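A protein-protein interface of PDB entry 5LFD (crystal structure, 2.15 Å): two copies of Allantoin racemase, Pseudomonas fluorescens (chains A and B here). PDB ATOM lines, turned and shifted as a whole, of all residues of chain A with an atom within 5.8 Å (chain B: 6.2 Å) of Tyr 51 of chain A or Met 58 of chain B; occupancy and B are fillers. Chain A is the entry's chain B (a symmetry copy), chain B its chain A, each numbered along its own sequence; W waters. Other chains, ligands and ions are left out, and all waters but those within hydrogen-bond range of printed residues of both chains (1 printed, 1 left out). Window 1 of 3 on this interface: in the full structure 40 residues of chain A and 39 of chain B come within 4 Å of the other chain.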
ATOM      1  N   GLY A  46      -3.604  -6.286  23.837  1.00  0.00           N
ATOM      2  CA  GLY A  46      -2.649  -7.285  24.336  1.00  0.00           C
ATOM      3  C   GLY A  46      -1.218  -6.903  24.087  1.00  0.00           C
ATOM      4  O   GLY A  46      -0.920  -5.967  23.342  1.00  0.00           O
ATOM      5  N   ASN A  47      -0.328  -7.639  24.732  1.00  0.00           N
ATOM      6  CA  ASN A  47       1.101  -7.379  24.657  1.00  0.00           C
ATOM      7  C   ASN A  47       1.625  -7.421  23.225  1.00  0.00           C
ATOM      8  O   ASN A  47       2.333  -6.509  22.817  1.00  0.00           O
ATOM      9  CB  ASN A  47       1.875  -8.329  25.587  1.00  0.00           C
ATOM     10  CG  ASN A  47       1.382  -8.250  27.021  1.00  0.00           C
ATOM     11  OD1 ASN A  47       1.732  -7.313  27.769  1.00  0.00           O
ATOM     12  ND2 ASN A  47       0.529  -9.192  27.397  1.00  0.00           N
ATOM     13  N   PHE A  48       1.290  -8.468  22.459  1.00  0.00           N
ATOM     14  CA  PHE A  48       1.847  -8.556  21.095  1.00  0.00           C
ATOM     15  C   PHE A  48       1.441  -7.303  20.318  1.00  0.00           C
ATOM     16  O   PHE A  48       2.264  -6.626  19.735  1.00  0.00           O
ATOM     17  CB  PHE A  48       1.405  -9.818  20.338  1.00  0.00           C
ATOM     18  CG  PHE A  48       1.502  -9.691  18.801  1.00  0.00           C
ATOM     19  CD1 PHE A  48       2.746  -9.636  18.164  1.00  0.00           C
ATOM     20  CD2 PHE A  48       0.353  -9.627  18.000  1.00  0.00           C
ATOM     21  CE1 PHE A  48       2.859  -9.504  16.775  1.00  0.00           C
ATOM     22  CE2 PHE A  48       0.457  -9.509  16.620  1.00  0.00           C
ATOM     23  CZ  PHE A  48       1.704  -9.451  16.012  1.00  0.00           C
ATOM     24  N   GLU A  49       0.157  -7.004  20.310  1.00  0.00           N
ATOM     25  CA  GLU A  49      -0.325  -5.879  19.502  1.00  0.00           C
ATOM     26  C   GLU A  49       0.205  -4.508  20.021  1.00  0.00           C
ATOM     27  O   GLU A  49       0.475  -3.562  19.254  1.00  0.00           O
ATOM     28  CB  GLU A  49      -1.851  -5.952  19.461  1.00  0.00           C
ATOM     29  CG  GLU A  49      -2.341  -7.081  18.557  1.00  0.00           C
ATOM     30  CD  GLU A  49      -3.788  -7.452  18.798  1.00  0.00           C
ATOM     31  OE1 GLU A  49      -4.506  -6.668  19.471  1.00  0.00           O
ATOM     32  OE2 GLU A  49      -4.232  -8.536  18.305  1.00  0.00           O
ATOM     33  N   SER A  50       0.377  -4.415  21.333  1.00  0.00           N
ATOM     34  CA  SER A  50       0.967  -3.251  21.936  1.00  0.00           C
ATOM     35  C   SER A  50       2.447  -2.985  21.514  1.00  0.00           C
ATOM     36  O   SER A  50       2.845  -1.840  21.255  1.00  0.00           O
ATOM     37  CB  SER A  50       0.793  -3.372  23.452  1.00  0.00           C
ATOM     38  OG  SER A  50       1.561  -2.375  24.059  1.00  0.00           O
ATOM     39  N   TYR A  51       3.258  -4.023  21.446  1.00  0.00           N
ATOM     40  CA  TYR A  51       4.620  -3.882  21.047  1.00  0.00           C
ATOM     41  C   TYR A  51       4.682  -3.593  19.536  1.00  0.00           C
ATOM     42  O   TYR A  51       5.585  -2.881  19.054  1.00  0.00           O
ATOM     43  CB  TYR A  51       5.394  -5.175  21.346  1.00  0.00           C
ATOM     44  CG  TYR A  51       5.838  -5.355  22.818  1.00  0.00           C
ATOM     45  CD1 TYR A  51       6.647  -4.386  23.436  1.00  0.00           C
ATOM     46  CD2 TYR A  51       5.534  -6.535  23.540  1.00  0.00           C
ATOM     47  CE1 TYR A  51       7.103  -4.558  24.743  1.00  0.00           C
ATOM     48  CE2 TYR A  51       5.977  -6.721  24.858  1.00  0.00           C
ATOM     49  CZ  TYR A  51       6.766  -5.712  25.469  1.00  0.00           C
ATOM     50  OH  TYR A  51       7.247  -5.836  26.776  1.00  0.00           O
ATOM     51  N   LEU A  52       3.763  -4.182  18.772  1.00  0.00           N
ATOM     52  CA  LEU A  52       3.701  -3.841  17.322  1.00  0.00           C
ATOM     53  C   LEU A  52       3.313  -2.365  17.183  1.00  0.00           C
ATOM     54  O   LEU A  52       3.913  -1.620  16.452  1.00  0.00           O
ATOM     55  CB  LEU A  52       2.703  -4.727  16.595  1.00  0.00           C
ATOM     56  CG  LEU A  52       2.815  -4.497  15.063  1.00  0.00           C
ATOM     57  CD1 LEU A  52       4.193  -4.694  14.398  1.00  0.00           C
ATOM     58  CD2 LEU A  52       1.834  -5.348  14.354  1.00  0.00           C
ATOM     59  N   ALA A  53       2.356  -1.928  17.986  1.00  0.00           N
ATOM     60  CA  ALA A  53       1.929  -0.519  17.978  1.00  0.00           C
ATOM     61  C   ALA A  53       2.992   0.449  18.437  1.00  0.00           C
ATOM     62  O   ALA A  53       3.057   1.585  17.912  1.00  0.00           O
ATOM     63  CB  ALA A  53       0.652  -0.322  18.818  1.00  0.00           C
ATOM     64  N   ALA A  54       3.784   0.069  19.439  1.00  0.00           N
ATOM     65  CA  ALA A  54       4.939   0.900  19.799  1.00  0.00           C
ATOM     66  C   ALA A  54       5.780   1.220  18.551  1.00  0.00           C
ATOM     67  O   ALA A  54       6.075   2.383  18.313  1.00  0.00           O
ATOM     68  CB  ALA A  54       5.830   0.297  20.924  1.00  0.00           C
ATOM     69  N   ILE A  55       6.171   0.246  17.747  1.00  0.00           N
ATOM     70  CA  ILE A  55       7.034   0.626  16.650  1.00  0.00           C
ATOM     71  C   ILE A  55       6.296   1.186  15.446  1.00  0.00           C
ATOM     72  O   ILE A  55       6.879   1.967  14.669  1.00  0.00           O
ATOM     73  CB  ILE A  55       8.052  -0.451  16.183  1.00  0.00           C
ATOM     74  CG1 ILE A  55       7.380  -1.624  15.509  1.00  0.00           C
ATOM     75  CG2 ILE A  55       8.905  -0.937  17.331  1.00  0.00           C
ATOM     76  CD1 ILE A  55       8.398  -2.701  15.188  1.00  0.00           C
ATOM     77  N   ALA A  56       5.041   0.804  15.300  1.00  0.00           N
ATOM     78  CA  ALA A  56       4.130   1.426  14.340  1.00  0.00           C
ATOM     79  C   ALA A  56       4.042   2.969  14.510  1.00  0.00           C
ATOM     80  O   ALA A  56       4.314   3.747  13.558  1.00  0.00           O
ATOM     81  CB  ALA A  56       2.759   0.788  14.468  1.00  0.00           C
ATOM     82  N   HIS A  79       2.696   0.376  24.866  1.00  0.00           N
ATOM     83  CA  HIS A  79       4.124   0.606  24.900  1.00  0.00           C
ATOM     84  C   HIS A  79       4.519   1.715  23.931  1.00  0.00           C
ATOM     85  O   HIS A  79       3.748   2.070  23.026  1.00  0.00           O
ATOM     86  CB  HIS A  79       4.828  -0.687  24.458  1.00  0.00           C
ATOM     87  CG  HIS A  79       4.737  -1.799  25.442  1.00  0.00           C
ATOM     88  ND1 HIS A  79       3.884  -2.873  25.277  1.00  0.00           N
ATOM     89  CD2 HIS A  79       5.364  -1.989  26.633  1.00  0.00           C
ATOM     90  CE1 HIS A  79       3.994  -3.680  26.324  1.00  0.00           C
ATOM     91  NE2 HIS A  79       4.891  -3.167  27.160  1.00  0.00           N
ATOM     92  N   TYR B  51      12.533  -1.737  21.752  1.00  0.00           N
ATOM     93  CA  TYR B  51      11.190  -1.998  21.205  1.00  0.00           C
ATOM     94  C   TYR B  51      11.291  -2.577  19.782  1.00  0.00           C
ATOM     95  O   TYR B  51      10.523  -3.456  19.377  1.00  0.00           O
ATOM     96  CB  TYR B  51      10.368  -0.710  21.172  1.00  0.00           C
ATOM     97  CG  TYR B  51       9.727  -0.310  22.520  1.00  0.00           C
ATOM     98  CD1 TYR B  51       8.844  -1.180  23.197  1.00  0.00           C
ATOM     99  CD2 TYR B  51       9.949   0.963  23.068  1.00  0.00           C
ATOM    100  CE1 TYR B  51       8.244  -0.807  24.377  1.00  0.00           C
ATOM    101  CE2 TYR B  51       9.347   1.353  24.265  1.00  0.00           C
ATOM    102  CZ  TYR B  51       8.498   0.475  24.913  1.00  0.00           C
ATOM    103  OH  TYR B  51       7.907   0.892  26.095  1.00  0.00           O
ATOM    104  N   ALA B  53      13.740  -4.409  18.709  1.00  0.00           N
ATOM    105  CA  ALA B  53      14.225  -5.782  18.946  1.00  0.00           C
ATOM    106  C   ALA B  53      13.102  -6.671  19.453  1.00  0.00           C
ATOM    107  O   ALA B  53      13.050  -7.851  19.126  1.00  0.00           O
ATOM    108  CB  ALA B  53      15.385  -5.786  19.940  1.00  0.00           C
ATOM    109  N   ALA B  54      12.187  -6.116  20.240  1.00  0.00           N
ATOM    110  CA  ALA B  54      11.065  -6.931  20.755  1.00  0.00           C
ATOM    111  C   ALA B  54      10.333  -7.564  19.599  1.00  0.00           C
ATOM    112  O   ALA B  54      10.008  -8.741  19.598  1.00  0.00           O
ATOM    113  CB  ALA B  54      10.088  -6.080  21.598  1.00  0.00           C
ATOM    114  N   ILE B  55      10.015  -6.737  18.621  1.00  0.00           N
ATOM    115  CA  ILE B  55       9.153  -7.109  17.533  1.00  0.00           C
ATOM    116  C   ILE B  55      10.009  -7.925  16.520  1.00  0.00           C
ATOM    117  O   ILE B  55       9.532  -8.884  15.942  1.00  0.00           O
ATOM    118  CB  ILE B  55       8.499  -5.801  16.991  1.00  0.00           C
ATOM    119  CG1 ILE B  55       7.101  -5.610  17.581  1.00  0.00           C
ATOM    120  CG2 ILE B  55       8.494  -5.719  15.482  1.00  0.00           C
ATOM    121  CD1 ILE B  55       6.185  -6.788  17.392  1.00  0.00           C
ATOM    122  N   ALA B  56      11.280  -7.574  16.386  1.00  0.00           N
ATOM    123  CA  ALA B  56      12.210  -8.295  15.522  1.00  0.00           C
ATOM    124  C   ALA B  56      12.391  -9.756  15.988  1.00  0.00           C
ATOM    125  O   ALA B  56      12.389 -10.703  15.178  1.00  0.00           O
ATOM    126  CB  ALA B  56      13.534  -7.587  15.474  1.00  0.00           C
ATOM    127  N   VAL B  57      12.496  -9.934  17.304  1.00  0.00           N
ATOM    128  CA  VAL B  57      12.524 -11.268  17.922  1.00  0.00           C
ATOM    129  C   VAL B  57      11.246 -12.049  17.659  1.00  0.00           C
ATOM    130  O   VAL B  57      11.322 -13.216  17.320  1.00  0.00           O
ATOM    131  CB  VAL B  57      12.800 -11.139  19.419  1.00  0.00           C
ATOM    132  CG1 VAL B  57      12.385 -12.376  20.183  1.00  0.00           C
ATOM    133  CG2 VAL B  57      14.265 -10.799  19.610  1.00  0.00           C
ATOM    134  N   MET B  58      10.081 -11.412  17.799  1.00  0.00           N
ATOM    135  CA  MET B  58       8.836 -12.140  17.651  1.00  0.00           C
ATOM    136  C   MET B  58       8.702 -12.568  16.177  1.00  0.00           C
ATOM    137  O   MET B  58       8.327 -13.692  15.873  1.00  0.00           O
ATOM    138  CB  MET B  58       7.627 -11.285  18.056  1.00  0.00           C
ATOM    139  CG  MET B  58       7.481 -10.948  19.522  1.00  0.00           C
ATOM    140  SD  MET B  58       6.035  -9.925  19.927  1.00  0.00           S
ATOM    141  CE  MET B  58       6.940  -8.611  20.752  1.00  0.00           C
ATOM    142  N   ASP B  59       9.003 -11.651  15.267  1.00  0.00           N
ATOM    143  CA  ASP B  59       8.919 -11.920  13.841  1.00  0.00           C
ATOM    144  C   ASP B  59       9.817 -13.148  13.565  1.00  0.00           C
ATOM    145  O   ASP B  59       9.357 -14.136  13.002  1.00  0.00           O
ATOM    146  CB  ASP B  59       9.324 -10.655  13.056  1.00  0.00           C
ATOM    147  CG  ASP B  59       9.604 -10.927  11.565  1.00  0.00           C
ATOM    148  OD1 ASP B  59      10.770 -10.820  11.054  1.00  0.00           O
ATOM    149  OD2 ASP B  59       8.628 -11.282  10.909  1.00  0.00           O
ATOM    150  N   ARG B  60      11.073 -13.112  13.996  1.00  0.00           N
ATOM    151  CA  ARG B  60      11.983 -14.209  13.751  1.00  0.00           C
ATOM    152  C   ARG B  60      11.401 -15.560  14.244  1.00  0.00           C
ATOM    153  O   ARG B  60      11.535 -16.569  13.578  1.00  0.00           O
ATOM    154  CB  ARG B  60      13.367 -13.885  14.370  1.00  0.00           C
ATOM    155  CG  ARG B  60      14.516 -14.819  13.992  1.00  0.00           C
ATOM    156  CD  ARG B  60      14.744 -14.914  12.473  1.00  0.00           C
ATOM    157  NE  ARG B  60      15.613 -16.042  12.075  1.00  0.00           N
ATOM    158  CZ  ARG B  60      15.143 -17.246  11.736  1.00  0.00           C
ATOM    159  NH1 ARG B  60      13.831 -17.509  11.781  1.00  0.00           N
ATOM    160  NH2 ARG B  60      15.994 -18.204  11.356  1.00  0.00           N
ATOM    161  N   VAL B  61      10.691 -15.552  15.377  1.00  0.00           N
ATOM    162  CA  VAL B  61      10.238 -16.785  15.992  1.00  0.00           C
ATOM    163  C   VAL B  61       9.054 -17.275  15.208  1.00  0.00           C
ATOM    164  O   VAL B  61       8.899 -18.494  15.049  1.00  0.00           O
ATOM    165  CB  VAL B  61       9.866 -16.593  17.501  1.00  0.00           C
ATOM    166  CG1 VAL B  61       8.921 -17.663  18.009  1.00  0.00           C
ATOM    167  CG2 VAL B  61      11.132 -16.476  18.374  1.00  0.00           C
ATOM    168  N   MET B  62       8.205 -16.349  14.745  1.00  0.00           N
ATOM    169  CA  MET B  62       6.984 -16.706  14.064  1.00  0.00           C
ATOM    170  C   MET B  62       7.299 -17.183  12.649  1.00  0.00           C
ATOM    171  O   MET B  62       6.476 -17.806  12.017  1.00  0.00           O
ATOM    172  CB  MET B  62       6.006 -15.532  14.035  1.00  0.00           C
ATOM    173  CG  MET B  62       5.362 -15.228  15.393  1.00  0.00           C
ATOM    174  SD  MET B  62       4.486 -16.623  16.183  1.00  0.00           S
ATOM    175  CE  MET B  62       5.675 -17.188  17.361  1.00  0.00           C
ATOM    176  N   ALA B  63       8.496 -16.865  12.157  1.00  0.00           N
ATOM    177  CA  ALA B  63       8.939 -17.284  10.832  1.00  0.00           C
ATOM    178  C   ALA B  63       9.509 -18.703  10.867  1.00  0.00           C
ATOM    179  O   ALA B  63       9.603 -19.353   9.836  1.00  0.00           O
ATOM    180  CB  ALA B  63       9.969 -16.302  10.264  1.00  0.00           C
ATOM    181  N   GLU B  78      15.725  -6.190  27.707  1.00  0.00           N
ATOM    182  CA  GLU B  78      14.916  -5.776  26.559  1.00  0.00           C
ATOM    183  C   GLU B  78      13.459  -6.121  26.706  1.00  0.00           C
ATOM    184  O   GLU B  78      13.091  -7.026  27.477  1.00  0.00           O
ATOM    185  CB  GLU B  78      15.443  -6.383  25.258  1.00  0.00           C
ATOM    186  CG  GLU B  78      16.511  -5.513  24.654  1.00  0.00           C
ATOM    187  CD  GLU B  78      17.881  -5.809  25.238  1.00  0.00           C
ATOM    188  OE1 GLU B  78      18.072  -6.995  25.625  1.00  0.00           O
ATOM    189  OE2 GLU B  78      18.728  -4.877  25.356  1.00  0.00           O
ATOM    190  N   HIS B  79      12.654  -5.383  25.948  1.00  0.00           N
ATOM    191  CA  HIS B  79      11.228  -5.615  25.756  1.00  0.00           C
ATOM    192  C   HIS B  79      10.960  -6.895  24.956  1.00  0.00           C
ATOM    193  O   HIS B  79      11.878  -7.406  24.330  1.00  0.00           O
ATOM    194  CB  HIS B  79      10.601  -4.379  25.078  1.00  0.00           C
ATOM    195  CG  HIS B  79      10.546  -3.168  25.978  1.00  0.00           C
ATOM    196  ND1 HIS B  79      11.380  -2.066  25.821  1.00  0.00           N
ATOM    197  CD2 HIS B  79       9.789  -2.910  27.076  1.00  0.00           C
ATOM    198  CE1 HIS B  79      11.090  -1.163  26.744  1.00  0.00           C
ATOM    199  NE2 HIS B  79      10.143  -1.659  27.529  1.00  0.00           N
ATOM    200  N   GLY B  80       9.732  -7.413  25.026  1.00  0.00           N
ATOM    201  CA  GLY B  80       9.267  -8.519  24.164  1.00  0.00           C
ATOM    202  C   GLY B  80       8.747  -9.843  24.752  1.00  0.00           C
ATOM    203  O   GLY B  80       7.861 -10.497  24.136  1.00  0.00           O
ATOM    204  N   ARG B  81       9.250 -10.243  25.933  1.00  0.00           N
ATOM    205  CA  ARG B  81       8.860 -11.520  26.528  1.00  0.00           C
ATOM    206  C   ARG B  81       7.330 -11.743  26.461  1.00  0.00           C
ATOM    207  O   ARG B  81       6.858 -12.779  26.012  1.00  0.00           O
ATOM    208  CB  ARG B  81       9.370 -11.646  27.988  1.00  0.00           C
ATOM    209  CG  ARG B  81       8.368 -12.382  28.882  1.00  0.00           C
ATOM    210  CD  ARG B  81       8.784 -12.591  30.324  1.00  0.00           C
ATOM    211  NE  ARG B  81       8.543 -11.442  31.197  1.00  0.00           N
ATOM    212  CZ  ARG B  81       7.355 -11.071  31.677  1.00  0.00           C
ATOM    213  NH1 ARG B  81       6.268 -11.729  31.351  1.00  0.00           N
ATOM    214  NH2 ARG B  81       7.253 -10.004  32.478  1.00  0.00           N
ATOM    215  N   GLU B  82       6.575 -10.757  26.914  1.00  0.00           N
ATOM    216  CA  GLU B  82       5.128 -10.841  27.065  1.00  0.00           C
ATOM    217  C   GLU B  82       4.475 -11.050  25.704  1.00  0.00           C
ATOM    218  O   GLU B  82       3.424 -11.664  25.611  1.00  0.00           O
ATOM    219  CB  GLU B  82       4.536  -9.548  27.655  1.00  0.00           C
ATOM    220  CG  GLU B  82       5.022  -9.085  29.016  1.00  0.00           C
ATOM    221  CD  GLU B  82       6.100  -8.022  28.887  1.00  0.00           C
ATOM    222  OE1 GLU B  82       6.906  -8.075  27.921  1.00  0.00           O
ATOM    223  OE2 GLU B  82       6.162  -7.143  29.793  1.00  0.00           O
ATOM    224  N   GLY B  83       5.100 -10.448  24.682  1.00  0.00           N
ATOM    225  CA  GLY B  83       4.600 -10.537  23.300  1.00  0.00           C
ATOM    226  C   GLY B  83       4.649 -11.973  22.872  1.00  0.00           C
ATOM    227  O   GLY B  83       3.629 -12.560  22.455  1.00  0.00           O
ATOM    228  N   LEU B  84       5.837 -12.538  23.016  1.00  0.00           N
ATOM    229  CA  LEU B  84       6.104 -13.975  22.771  1.00  0.00           C
ATOM    230  C   LEU B  84       5.199 -14.886  23.572  1.00  0.00           C
ATOM    231  O   LEU B  84       4.717 -15.894  23.043  1.00  0.00           O
ATOM    232  CB  LEU B  84       7.553 -14.316  23.165  1.00  0.00           C
ATOM    233  CG  LEU B  84       8.758 -14.465  22.218  1.00  0.00           C
ATOM    234  CD1 LEU B  84       8.584 -14.265  20.704  1.00  0.00           C
ATOM    235  CD2 LEU B  84       9.974 -13.734  22.771  1.00  0.00           C
ATOM    236  N   LEU B  87       1.822 -15.020  21.874  1.00  0.00           N
ATOM    237  CA  LEU B  87       1.833 -15.688  20.555  1.00  0.00           C
ATOM    238  C   LEU B  87       2.095 -17.224  20.609  1.00  0.00           C
ATOM    239  O   LEU B  87       1.690 -17.952  19.720  1.00  0.00           O
ATOM    240  CB  LEU B  87       2.886 -15.029  19.666  1.00  0.00           C
ATOM    241  CG  LEU B  87       2.724 -13.614  19.135  1.00  0.00           C
ATOM    242  CD1 LEU B  87       4.092 -13.126  18.664  1.00  0.00           C
ATOM    243  CD2 LEU B  87       1.677 -13.526  18.010  1.00  0.00           C
ATOM    244  N   ARG B 126      12.823  -3.854  33.861  1.00  0.00           N
ATOM    245  CA  ARG B 126      12.375  -5.215  33.523  1.00  0.00           C
ATOM    246  C   ARG B 126      12.245  -6.051  34.840  1.00  0.00           C
ATOM    247  O   ARG B 126      11.254  -6.746  35.078  1.00  0.00           O
ATOM    248  CB  ARG B 126      13.270  -5.900  32.468  1.00  0.00           C
ATOM    249  CG  ARG B 126      13.306  -5.251  31.080  1.00  0.00           C
ATOM    250  CD  ARG B 126      11.904  -5.077  30.492  1.00  0.00           C
ATOM    251  NE  ARG B 126      11.248  -6.362  30.314  1.00  0.00           N
ATOM    252  CZ  ARG B 126       9.974  -6.483  29.944  1.00  0.00           C
ATOM    253  NH1 ARG B 126       9.254  -5.386  29.716  1.00  0.00           N
ATOM    254  NH2 ARG B 126       9.436  -7.674  29.758  1.00  0.00           N
ATOM    255  N   LEU B 129       9.123  -5.075  36.847  1.00  0.00           N
ATOM    256  CA  LEU B 129       7.906  -5.671  36.240  1.00  0.00           C
ATOM    257  C   LEU B 129       7.753  -7.141  36.547  1.00  0.00           C
ATOM    258  O   LEU B 129       6.647  -7.652  36.561  1.00  0.00           O
ATOM    259  CB  LEU B 129       7.921  -5.604  34.695  1.00  0.00           C
ATOM    260  CG  LEU B 129       7.425  -4.319  34.030  1.00  0.00           C
ATOM    261  CD1 LEU B 129       7.938  -4.293  32.578  1.00  0.00           C
ATOM    262  CD2 LEU B 129       5.896  -4.287  34.088  1.00  0.00           C
HETATM  263  O   HOH W   1       8.026  -3.031  20.334  1.00  0.00           O
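NE of Arg 126 of chain B is in hydrogen-bond range of O of Glu 78 of chain B.
OE1 of Glu 82 of chain B lies within salt-bridge range of NH2 of Arg 126 of chain B, 3.2 Å away.
The side-chain hydroxyl (OG) of Ser 50 of chain A sits at hydrogen-bond distance from a ring nitrogen (ND1) of His 79 of chain A.
Among the printed residues, merely in contact across the chains: Asn 47 of chain A with Glu 82 of chain B, Asn 47 of chain A with Gly 83 of chain B, Phe 48 of chain A with Met 58 of chain B, Phe 48 of chain A with Gly 83 of chain B, Phe 48 of chain A with Leu 87 of chain B, Tyr 51 of chain A with Tyr 51 of chain B, Tyr 51 of chain A with Ile 55 of chain B, Tyr 51 of chain A with Met 58 of chain B, Tyr 51 of chain A with His 79 of chain B, Tyr 51 of chain A with Gly 83 of chain B, Tyr 51 of chain A with Arg 126 of chain B, Leu 52 of chain A with Ile 55 of chain B, Ile 55 of chain A with Tyr 51 of chain B, Ile 55 of chain A with Ile 55 of chain B and His 79 of chain A with Tyr 51 of chain B.
Tyr 51 of chain A touches just these residues of chain B: Tyr 51 (3.9 Å), Ile 55 (3.5 Å), Met 58 (3.7 Å), His 79 (3.5 Å), Gly 80 (3.4 Å), Glu 82 (2.5 Å), Gly 83 (3.8 Å) and Arg 126 (3.6 Å).
Met 58 of chain B touches just these residues of chain A: Phe 48 and Tyr 51.
Of the printed residues of chain B, His 79 of chain A touches Tyr 51 (3.4 Å).
Printed residues of chain A within 4 Å of Ile 55 of chain B: Tyr 51 (3.5 Å), Leu 52 (3.8 Å) and Ile 55 (3.0 Å).
Of the printed residues of chain A, His 79 of chain B touches Tyr 51 (3.5 Å).
Of the printed residues of chain B, Phe 48 of chain A touches Met 58, Gly 83 and Leu 87.
The nearest residue of chain B that does not touch Tyr 51 of chain A is Ala 54 of chain B (4.3 Å).
The nearest residue of chain A that does not touch Met 58 of chain B is Asn 47 of chain A (5.5 Å).
Tyr 51 of chain A touches its own counterpart, Tyr 51 of chain B.
Tyr 51 of chain A touches Ile 55 of chain B, and with the chains exchanged Ile 55 of chain A touches Tyr 51 of chain B.
Tyr 51 of chain A touches His 79 of chain B, and with the chains exchanged His 79 of chain A touches Tyr 51 of chain B.
Ile 55 of chain B touches its own counterpart, Ile 55 of chain A.
Of the 17 pairs that touch across the chains among the printed residues, 6 have their exchanged pair printed and touching as well.
N of Gly 80 of chain B is in hydrogen-bond range of OH of Tyr 51 of chain A (3.4 Å).
OH of Tyr 51 of chain A lies within hydrogen-bond range of OE1 of Glu 82 of chain B, at 2.5 Å.
Water W1 lies within hydrogen-bond range of O of Tyr 51 of chain B and O of Tyr 51 of chain A.
Hydrophobic or aromatic side chains of chain B within 4 Å of the printed part of chain A: Tyr 51, Ile 55, Met 58, His 79 and Leu 87.
Printed residues of chain A that touch a printed residue of chain B: Asn 47, Phe 48, Tyr 51, Leu 52, Ile 55 and His 79.
Hydrophobic or aromatic side chains of chain A within 4 Å of the printed part of chain B: Phe 48, Tyr 51, Ile 55 and His 79.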
